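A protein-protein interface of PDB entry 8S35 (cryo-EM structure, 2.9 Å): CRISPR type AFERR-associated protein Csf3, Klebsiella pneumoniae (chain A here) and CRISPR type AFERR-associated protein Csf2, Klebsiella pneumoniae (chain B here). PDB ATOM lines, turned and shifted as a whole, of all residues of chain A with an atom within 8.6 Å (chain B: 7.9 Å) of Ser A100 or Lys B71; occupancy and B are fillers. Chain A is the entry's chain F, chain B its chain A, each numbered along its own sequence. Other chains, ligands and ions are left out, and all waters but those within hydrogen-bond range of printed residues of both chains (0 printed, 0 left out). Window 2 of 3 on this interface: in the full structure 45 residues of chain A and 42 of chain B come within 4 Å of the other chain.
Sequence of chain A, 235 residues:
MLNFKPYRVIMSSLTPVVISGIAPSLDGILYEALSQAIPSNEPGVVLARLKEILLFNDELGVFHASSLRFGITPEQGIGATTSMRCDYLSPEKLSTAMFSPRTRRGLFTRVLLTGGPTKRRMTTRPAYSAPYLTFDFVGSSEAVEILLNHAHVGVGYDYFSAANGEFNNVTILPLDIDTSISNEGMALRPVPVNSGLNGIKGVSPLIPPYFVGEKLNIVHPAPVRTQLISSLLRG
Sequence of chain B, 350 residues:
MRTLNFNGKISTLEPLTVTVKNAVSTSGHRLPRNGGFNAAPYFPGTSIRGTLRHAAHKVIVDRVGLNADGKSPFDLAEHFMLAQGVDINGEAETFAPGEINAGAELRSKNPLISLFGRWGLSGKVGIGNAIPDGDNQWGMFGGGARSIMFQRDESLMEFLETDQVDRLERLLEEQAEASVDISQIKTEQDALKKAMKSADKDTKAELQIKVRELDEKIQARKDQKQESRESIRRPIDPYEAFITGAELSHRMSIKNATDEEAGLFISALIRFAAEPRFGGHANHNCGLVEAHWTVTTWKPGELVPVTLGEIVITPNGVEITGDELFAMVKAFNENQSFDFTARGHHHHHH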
ATOM      1  N   LYS A  93     -14.734 -10.713 -17.725  1.00  0.00           N
ATOM      2  CA  LYS A  93     -15.776 -11.525 -18.341  1.00  0.00           C
ATOM      3  C   LYS A  93     -15.286 -12.946 -18.573  1.00  0.00           C
ATOM      4  O   LYS A  93     -16.025 -13.912 -18.353  1.00  0.00           O
ATOM      5  CB  LYS A  93     -16.224 -10.893 -19.658  1.00  0.00           C
ATOM      6  CG  LYS A  93     -17.144  -9.699 -19.486  1.00  0.00           C
ATOM      7  CD  LYS A  93     -17.525  -9.101 -20.827  1.00  0.00           C
ATOM      8  CE  LYS A  93     -18.394  -7.870 -20.661  1.00  0.00           C
ATOM      9  NZ  LYS A  93     -19.030  -7.463 -21.944  1.00  0.00           N
ATOM     10  N   SER A  95     -13.431 -15.134 -16.952  1.00  0.00           N
ATOM     11  CA  SER A  95     -12.841 -15.590 -15.703  1.00  0.00           C
ATOM     12  C   SER A  95     -13.803 -16.537 -15.006  1.00  0.00           C
ATOM     13  O   SER A  95     -15.022 -16.424 -15.149  1.00  0.00           O
ATOM     14  CB  SER A  95     -12.503 -14.414 -14.781  1.00  0.00           C
ATOM     15  OG  SER A  95     -12.180 -14.871 -13.480  1.00  0.00           O
ATOM     16  N   THR A  96     -13.236 -17.470 -14.238  1.00  0.00           N
ATOM     17  CA  THR A  96     -14.060 -18.428 -13.512  1.00  0.00           C
ATOM     18  C   THR A  96     -14.881 -17.774 -12.412  1.00  0.00           C
ATOM     19  O   THR A  96     -15.848 -18.378 -11.938  1.00  0.00           O
ATOM     20  CB  THR A  96     -13.188 -19.523 -12.903  1.00  0.00           C
ATOM     21  OG1 THR A  96     -12.054 -18.931 -12.259  1.00  0.00           O
ATOM     22  CG2 THR A  96     -12.719 -20.482 -13.978  1.00  0.00           C
ATOM     23  N   ALA A  97     -14.523 -16.557 -11.999  1.00  0.00           N
ATOM     24  CA  ALA A  97     -15.309 -15.860 -10.991  1.00  0.00           C
ATOM     25  C   ALA A  97     -16.706 -15.524 -11.487  1.00  0.00           C
ATOM     26  O   ALA A  97     -17.595 -15.266 -10.669  1.00  0.00           O
ATOM     27  CB  ALA A  97     -14.594 -14.580 -10.560  1.00  0.00           C
ATOM     28  N   MET A  98     -16.918 -15.525 -12.805  1.00  0.00           N
ATOM     29  CA  MET A  98     -18.177 -15.112 -13.401  1.00  0.00           C
ATOM     30  C   MET A  98     -18.979 -16.261 -13.991  1.00  0.00           C
ATOM     31  O   MET A  98     -20.191 -16.115 -14.170  1.00  0.00           O
ATOM     32  CB  MET A  98     -17.906 -14.068 -14.491  1.00  0.00           C
ATOM     33  CG  MET A  98     -18.136 -12.642 -14.024  1.00  0.00           C
ATOM     34  SD  MET A  98     -18.073 -11.441 -15.358  1.00  0.00           S
ATOM     35  CE  MET A  98     -19.807 -11.292 -15.737  1.00  0.00           C
ATOM     36  N   PHE A  99     -18.345 -17.388 -14.301  1.00  0.00           N
ATOM     37  CA  PHE A  99     -19.047 -18.547 -14.839  1.00  0.00           C
ATOM     38  C   PHE A  99     -18.129 -19.758 -14.726  1.00  0.00           C
ATOM     39  O   PHE A  99     -16.970 -19.644 -14.320  1.00  0.00           O
ATOM     40  CB  PHE A  99     -19.494 -18.302 -16.280  1.00  0.00           C
ATOM     41  CG  PHE A  99     -18.384 -18.368 -17.281  1.00  0.00           C
ATOM     42  CD1 PHE A  99     -17.452 -17.352 -17.367  1.00  0.00           C
ATOM     43  CD2 PHE A  99     -18.278 -19.443 -18.142  1.00  0.00           C
ATOM     44  CE1 PHE A  99     -16.433 -17.409 -18.292  1.00  0.00           C
ATOM     45  CE2 PHE A  99     -17.261 -19.504 -19.069  1.00  0.00           C
ATOM     46  CZ  PHE A  99     -16.338 -18.485 -19.144  1.00  0.00           C
ATOM     47  N   SER A 100     -18.662 -20.928 -15.083  1.00  0.00           N
ATOM     48  CA  SER A 100     -17.964 -22.207 -14.943  1.00  0.00           C
ATOM     49  C   SER A 100     -17.710 -22.804 -16.322  1.00  0.00           C
ATOM     50  O   SER A 100     -18.571 -23.516 -16.862  1.00  0.00           O
ATOM     51  CB  SER A 100     -18.779 -23.170 -14.083  1.00  0.00           C
ATOM     52  OG  SER A 100     -19.025 -22.619 -12.801  1.00  0.00           O
ATOM     53  N   PRO A 101     -16.552 -22.551 -16.930  1.00  0.00           N
ATOM     54  CA  PRO A 101     -16.252 -23.193 -18.215  1.00  0.00           C
ATOM     55  C   PRO A 101     -16.074 -24.692 -18.059  1.00  0.00           C
ATOM     56  O   PRO A 101     -15.631 -25.184 -17.019  1.00  0.00           O
ATOM     57  CB  PRO A 101     -14.944 -22.530 -18.664  1.00  0.00           C
ATOM     58  CG  PRO A 101     -14.631 -21.481 -17.676  1.00  0.00           C
ATOM     59  CD  PRO A 101     -15.434 -21.720 -16.455  1.00  0.00           C
ATOM     60  N   ARG A 102     -16.429 -25.423 -19.112  1.00  0.00           N
ATOM     61  CA  ARG A 102     -16.183 -26.857 -19.119  1.00  0.00           C
ATOM     62  C   ARG A 102     -14.682 -27.115 -19.099  1.00  0.00           C
ATOM     63  O   ARG A 102     -13.913 -26.453 -19.800  1.00  0.00           O
ATOM     64  CB  ARG A 102     -16.826 -27.503 -20.346  1.00  0.00           C
ATOM     65  CG  ARG A 102     -18.345 -27.537 -20.285  1.00  0.00           C
ATOM     66  CD  ARG A 102     -18.912 -28.802 -20.909  1.00  0.00           C
ATOM     67  NE  ARG A 102     -18.382 -29.056 -22.243  1.00  0.00           N
ATOM     68  CZ  ARG A 102     -18.685 -28.349 -23.324  1.00  0.00           C
ATOM     69  NH1 ARG A 102     -19.513 -27.317 -23.271  1.00  0.00           N
ATOM     70  NH2 ARG A 102     -18.146 -28.688 -24.491  1.00  0.00           N
ATOM     71  N   THR A 103     -14.270 -28.082 -18.285  1.00  0.00           N
ATOM     72  CA  THR A 103     -12.865 -28.334 -18.002  1.00  0.00           C
ATOM     73  C   THR A 103     -12.428 -29.677 -18.572  1.00  0.00           C
ATOM     74  O   THR A 103     -13.177 -30.657 -18.530  1.00  0.00           O
ATOM     75  CB  THR A 103     -12.607 -28.312 -16.492  1.00  0.00           C
ATOM     76  OG1 THR A 103     -13.021 -27.050 -15.953  1.00  0.00           O
ATOM     77  CG2 THR A 103     -11.132 -28.530 -16.188  1.00  0.00           C
ATOM     78  N   ARG A 104     -11.211 -29.704 -19.108  1.00  0.00           N
ATOM     79  CA  ARG A 104     -10.577 -30.922 -19.591  1.00  0.00           C
ATOM     80  C   ARG A 104      -9.105 -30.855 -19.215  1.00  0.00           C
ATOM     81  O   ARG A 104      -8.455 -29.832 -19.443  1.00  0.00           O
ATOM     82  CB  ARG A 104     -10.753 -31.092 -21.105  1.00  0.00           C
ATOM     83  CG  ARG A 104      -9.983 -30.092 -21.952  1.00  0.00           C
ATOM     84  CD  ARG A 104     -10.431 -30.125 -23.407  1.00  0.00           C
ATOM     85  NE  ARG A 104     -10.302 -31.453 -24.002  1.00  0.00           N
ATOM     86  CZ  ARG A 104     -11.265 -32.366 -24.070  1.00  0.00           C
ATOM     87  NH1 ARG A 104     -12.473 -32.147 -23.572  1.00  0.00           N
ATOM     88  NH2 ARG A 104     -11.009 -33.532 -24.654  1.00  0.00           N
ATOM     89  N   GLY A 106      -8.083 -30.419 -16.395  1.00  0.00           N
ATOM     90  CA  GLY A 106      -7.974 -29.325 -15.458  1.00  0.00           C
ATOM     91  C   GLY A 106      -7.832 -27.964 -16.100  1.00  0.00           C
ATOM     92  O   GLY A 106      -7.754 -26.964 -15.376  1.00  0.00           O
ATOM     93  N   PHE A 108      -9.315 -24.884 -18.552  1.00  0.00           N
ATOM     94  CA  PHE A 108     -10.602 -24.318 -18.924  1.00  0.00           C
ATOM     95  C   PHE A 108     -10.631 -24.070 -20.424  1.00  0.00           C
ATOM     96  O   PHE A 108      -9.737 -23.417 -20.971  1.00  0.00           O
ATOM     97  CB  PHE A 108     -10.857 -23.024 -18.154  1.00  0.00           C
ATOM     98  CG  PHE A 108     -10.829 -23.201 -16.668  1.00  0.00           C
ATOM     99  CD1 PHE A 108     -11.748 -24.024 -16.040  1.00  0.00           C
ATOM    100  CD2 PHE A 108      -9.875 -22.561 -15.898  1.00  0.00           C
ATOM    101  CE1 PHE A 108     -11.721 -24.196 -14.673  1.00  0.00           C
ATOM    102  CE2 PHE A 108      -9.845 -22.729 -14.529  1.00  0.00           C
ATOM    103  CZ  PHE A 108     -10.768 -23.550 -13.917  1.00  0.00           C
ATOM    104  N   THR A 109     -11.657 -24.597 -21.083  1.00  0.00           N
ATOM    105  CA  THR A 109     -11.773 -24.495 -22.532  1.00  0.00           C
ATOM    106  C   THR A 109     -11.994 -23.038 -22.913  1.00  0.00           C
ATOM    107  O   THR A 109     -13.057 -22.473 -22.638  1.00  0.00           O
ATOM    108  CB  THR A 109     -12.918 -25.367 -23.034  1.00  0.00           C
ATOM    109  OG1 THR A 109     -14.153 -24.909 -22.468  1.00  0.00           O
ATOM    110  CG2 THR A 109     -12.699 -26.829 -22.651  1.00  0.00           C
ATOM    111  N   VAL B  64     -26.304 -14.152  -6.807  1.00  0.00           N
ATOM    112  CA  VAL B  64     -26.488 -15.588  -6.963  1.00  0.00           C
ATOM    113  C   VAL B  64     -25.474 -16.345  -6.119  1.00  0.00           C
ATOM    114  O   VAL B  64     -25.801 -17.359  -5.492  1.00  0.00           O
ATOM    115  CB  VAL B  64     -26.391 -15.971  -8.451  1.00  0.00           C
ATOM    116  CG1 VAL B  64     -26.292 -17.478  -8.610  1.00  0.00           C
ATOM    117  CG2 VAL B  64     -27.589 -15.429  -9.214  1.00  0.00           C
ATOM    118  N   GLY B  65     -24.234 -15.870  -6.091  1.00  0.00           N
ATOM    119  CA  GLY B  65     -23.197 -16.545  -5.344  1.00  0.00           C
ATOM    120  C   GLY B  65     -22.589 -17.689  -6.136  1.00  0.00           C
ATOM    121  O   GLY B  65     -22.701 -17.773  -7.363  1.00  0.00           O
ATOM    122  N   LEU B  66     -21.935 -18.586  -5.405  1.00  0.00           N
ATOM    123  CA  LEU B  66     -21.235 -19.722  -5.980  1.00  0.00           C
ATOM    124  C   LEU B  66     -21.870 -21.021  -5.504  1.00  0.00           C
ATOM    125  O   LEU B  66     -22.498 -21.083  -4.444  1.00  0.00           O
ATOM    126  CB  LEU B  66     -19.748 -19.704  -5.602  1.00  0.00           C
ATOM    127  CG  LEU B  66     -18.978 -18.440  -5.985  1.00  0.00           C
ATOM    128  CD1 LEU B  66     -17.673 -18.357  -5.210  1.00  0.00           C
ATOM    129  CD2 LEU B  66     -18.719 -18.404  -7.480  1.00  0.00           C
ATOM    130  N   ASN B  67     -21.694 -22.063  -6.310  1.00  0.00           N
ATOM    131  CA  ASN B  67     -22.221 -23.377  -5.982  1.00  0.00           C
ATOM    132  C   ASN B  67     -21.499 -23.938  -4.759  1.00  0.00           C
ATOM    133  O   ASN B  67     -20.551 -23.351  -4.232  1.00  0.00           O
ATOM    134  CB  ASN B  67     -22.073 -24.317  -7.178  1.00  0.00           C
ATOM    135  CG  ASN B  67     -23.113 -24.068  -8.250  1.00  0.00           C
ATOM    136  OD1 ASN B  67     -24.193 -23.545  -7.978  1.00  0.00           O
ATOM    137  ND2 ASN B  67     -22.792 -24.447  -9.481  1.00  0.00           N
ATOM    138  N   ALA B  68     -21.966 -25.102  -4.298  1.00  0.00           N
ATOM    139  CA  ALA B  68     -21.320 -25.762  -3.169  1.00  0.00           C
ATOM    140  C   ALA B  68     -19.870 -26.105  -3.485  1.00  0.00           C
ATOM    141  O   ALA B  68     -19.040 -26.190  -2.573  1.00  0.00           O
ATOM    142  CB  ALA B  68     -22.093 -27.023  -2.787  1.00  0.00           C
ATOM    143  N   ASP B  69     -19.548 -26.297  -4.762  1.00  0.00           N
ATOM    144  CA  ASP B  69     -18.187 -26.580  -5.191  1.00  0.00           C
ATOM    145  C   ASP B  69     -17.343 -25.321  -5.343  1.00  0.00           C
ATOM    146  O   ASP B  69     -16.162 -25.426  -5.691  1.00  0.00           O
ATOM    147  CB  ASP B  69     -18.208 -27.342  -6.518  1.00  0.00           C
ATOM    148  CG  ASP B  69     -17.052 -28.313  -6.653  1.00  0.00           C
ATOM    149  OD1 ASP B  69     -15.994 -28.074  -6.034  1.00  0.00           O
ATOM    150  OD2 ASP B  69     -17.201 -29.317  -7.381  1.00  0.00           O
ATOM    151  N   GLY B  70     -17.910 -24.142  -5.098  1.00  0.00           N
ATOM    152  CA  GLY B  70     -17.162 -22.912  -5.252  1.00  0.00           C
ATOM    153  C   GLY B  70     -16.987 -22.470  -6.685  1.00  0.00           C
ATOM    154  O   GLY B  70     -16.031 -21.751  -6.991  1.00  0.00           O
ATOM    155  N   LYS B  71     -17.886 -22.882  -7.573  1.00  0.00           N
ATOM    156  CA  LYS B  71     -17.858 -22.503  -8.977  1.00  0.00           C
ATOM    157  C   LYS B  71     -19.156 -21.793  -9.327  1.00  0.00           C
ATOM    158  O   LYS B  71     -20.223 -22.122  -8.800  1.00  0.00           O
ATOM    159  CB  LYS B  71     -17.666 -23.727  -9.878  1.00  0.00           C
ATOM    160  CG  LYS B  71     -16.342 -24.444  -9.664  1.00  0.00           C
ATOM    161  CD  LYS B  71     -16.289 -25.763 -10.415  1.00  0.00           C
ATOM    162  CE  LYS B  71     -16.109 -25.547 -11.907  1.00  0.00           C
ATOM    163  NZ  LYS B  71     -15.869 -26.825 -12.630  1.00  0.00           N
ATOM    164  N   SER B  72     -19.054 -20.810 -10.214  1.00  0.00           N
ATOM    165  CA  SER B  72     -20.219 -20.013 -10.564  1.00  0.00           C
ATOM    166  C   SER B  72     -21.279 -20.900 -11.218  1.00  0.00           C
ATOM    167  O   SER B  72     -20.944 -21.744 -12.057  1.00  0.00           O
ATOM    168  CB  SER B  72     -19.824 -18.884 -11.514  1.00  0.00           C
ATOM    169  OG  SER B  72     -19.249 -17.801 -10.806  1.00  0.00           O
ATOM    170  N   PRO B  73     -22.562 -20.747 -10.866  1.00  0.00           N
ATOM    171  CA  PRO B  73     -23.583 -21.603 -11.494  1.00  0.00           C
ATOM    172  C   PRO B  73     -23.738 -21.374 -12.984  1.00  0.00           C
ATOM    173  O   PRO B  73     -24.283 -22.245 -13.673  1.00  0.00           O
ATOM    174  CB  PRO B  73     -24.871 -21.236 -10.746  1.00  0.00           C
ATOM    175  CG  PRO B  73     -24.439 -20.550  -9.521  1.00  0.00           C
ATOM    176  CD  PRO B  73     -23.163 -19.865  -9.850  1.00  0.00           C
ATOM    177  N   PHE B  74     -23.282 -20.241 -13.505  1.00  0.00           N
ATOM    178  CA  PHE B  74     -23.494 -19.921 -14.907  1.00  0.00           C
ATOM    179  C   PHE B  74     -22.541 -20.708 -15.795  1.00  0.00           C
ATOM    180  O   PHE B  74     -21.361 -20.876 -15.475  1.00  0.00           O
ATOM    181  CB  PHE B  74     -23.301 -18.425 -15.145  1.00  0.00           C
ATOM    182  CG  PHE B  74     -24.153 -17.562 -14.267  1.00  0.00           C
ATOM    183  CD1 PHE B  74     -25.519 -17.753 -14.208  1.00  0.00           C
ATOM    184  CD2 PHE B  74     -23.587 -16.562 -13.501  1.00  0.00           C
ATOM    185  CE1 PHE B  74     -26.305 -16.965 -13.402  1.00  0.00           C
ATOM    186  CE2 PHE B  74     -24.370 -15.767 -12.692  1.00  0.00           C
ATOM    187  CZ  PHE B  74     -25.731 -15.970 -12.642  1.00  0.00           C
ATOM    188  N   ASP B  75     -23.069 -21.190 -16.912  1.00  0.00           N
ATOM    189  CA  ASP B  75     -22.292 -21.855 -17.941  1.00  0.00           C
ATOM    190  C   ASP B  75     -21.961 -20.837 -19.027  1.00  0.00           C
ATOM    191  O   ASP B  75     -22.260 -19.647 -18.903  1.00  0.00           O
ATOM    192  CB  ASP B  75     -23.053 -23.066 -18.488  1.00  0.00           C
ATOM    193  CG  ASP B  75     -24.395 -22.696 -19.094  1.00  0.00           C
ATOM    194  OD1 ASP B  75     -24.767 -21.506 -19.059  1.00  0.00           O
ATOM    195  OD2 ASP B  75     -25.080 -23.603 -19.610  1.00  0.00           O
ATOM    196  N   LEU B  76     -21.338 -21.301 -20.110  1.00  0.00           N
ATOM    197  CA  LEU B  76     -20.968 -20.387 -21.185  1.00  0.00           C
ATOM    198  C   LEU B  76     -22.200 -19.748 -21.812  1.00  0.00           C
ATOM    199  O   LEU B  76     -22.214 -18.542 -22.080  1.00  0.00           O
ATOM    200  CB  LEU B  76     -20.150 -21.124 -22.242  1.00  0.00           C
ATOM    201  CG  LEU B  76     -19.359 -20.228 -23.196  1.00  0.00           C
ATOM    202  CD1 LEU B  76     -18.176 -19.589 -22.487  1.00  0.00           C
ATOM    203  CD2 LEU B  76     -18.891 -21.018 -24.405  1.00  0.00           C
ATOM    204  N   ALA B  77     -23.249 -20.538 -22.046  1.00  0.00           N
ATOM    205  CA  ALA B  77     -24.454 -20.003 -22.672  1.00  0.00           C
ATOM    206  C   ALA B  77     -25.100 -18.935 -21.800  1.00  0.00           C
ATOM    207  O   ALA B  77     -25.362 -17.818 -22.260  1.00  0.00           O
ATOM    208  CB  ALA B  77     -25.442 -21.135 -22.955  1.00  0.00           C
ATOM    209  N   HIS B  79     -23.759 -17.345 -19.288  1.00  0.00           N
ATOM    210  CA  HIS B  79     -22.820 -16.255 -19.063  1.00  0.00           C
ATOM    211  C   HIS B  79     -22.844 -15.273 -20.223  1.00  0.00           C
ATOM    212  O   HIS B  79     -22.880 -14.056 -20.016  1.00  0.00           O
ATOM    213  CB  HIS B  79     -21.413 -16.810 -18.866  1.00  0.00           C
ATOM    214  CG  HIS B  79     -20.346 -15.760 -18.864  1.00  0.00           C
ATOM    215  ND1 HIS B  79     -20.077 -14.975 -17.764  1.00  0.00           N
ATOM    216  CD2 HIS B  79     -19.488 -15.360 -19.831  1.00  0.00           C
ATOM    217  CE1 HIS B  79     -19.093 -14.141 -18.052  1.00  0.00           C
ATOM    218  NE2 HIS B  79     -18.718 -14.353 -19.300  1.00  0.00           N
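The backbone NH (N) of Ser A100 lies within hydrogen-bond range of the backbone carbonyl oxygen (O) of Phe B74.
The side-chain hydroxyl of Ser A100 lies within hydrogen-bond range of the backbone NH of Ser B72 (3.2 Å).
The backbone carbonyl oxygen (O) of Lys A93 sits at hydrogen-bond distance from a ring nitrogen (NE2) of His B79 (2.9 Å).
The side-chain hydroxyl (OG) of Ser B72 lies within hydrogen-bond range of the backbone carbonyl oxygen (O) of Ala A97 (3.0 Å).
OG of Ser A95 lies close to N of Ala A97 (3.2 Å).
O of Thr A96 touches OG of Ser B72 (3.6 Å).
Met A98 touches Ser B72 (C to OG, 3.5 Å).
O of Met A98 touches CD2 of Phe B74 (3.5 Å).
His B79 touches Met A98 (CE1 to CE, 3.7 Å).
Ser B72 touches Phe A99 (CB to CA, 3.4 Å).
Phe A99 touches Phe B74 (CB to O, 3.3 Å).
Phe A99 touches Leu B76.
Phe A99 touches His B79.
Ser A100 touches Lys B71.
Of the printed residues of chain B, Thr A96 touches Ser B72 (3.6 Å).
Printed residues of chain B within 4 Å of Phe A99: Ser B72, Phe B74, Leu B76 and His B79.
Ser A100 touches just these residues of chain B: Lys B71, Ser B72 and Phe B74.
No residue of chain B comes within 4 Å of Pro A101.
No residue of chain A comes within 4 Å of Gly B70.
Of the printed residues of chain A, Lys B71 touches Ser A100.
The nearest residue of chain B that does not touch Ser A100 is Asp B75 (4.2 Å).
Printed residues of chain A that touch a printed residue of chain B: Lys A93, Thr A96, Ala A97, Met A98, Phe A99 and Ser A100.
Printed residues of chain B that touch a printed residue of chain A: Lys B71, Ser B72, Phe B74, Leu B76 and His B79.
Hydrophobic or aromatic side chains of chain B that line the printed part of chain A: Phe B74, Leu B76 and His B79.
Among the printed residues, 13 pairs touch across the chains.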
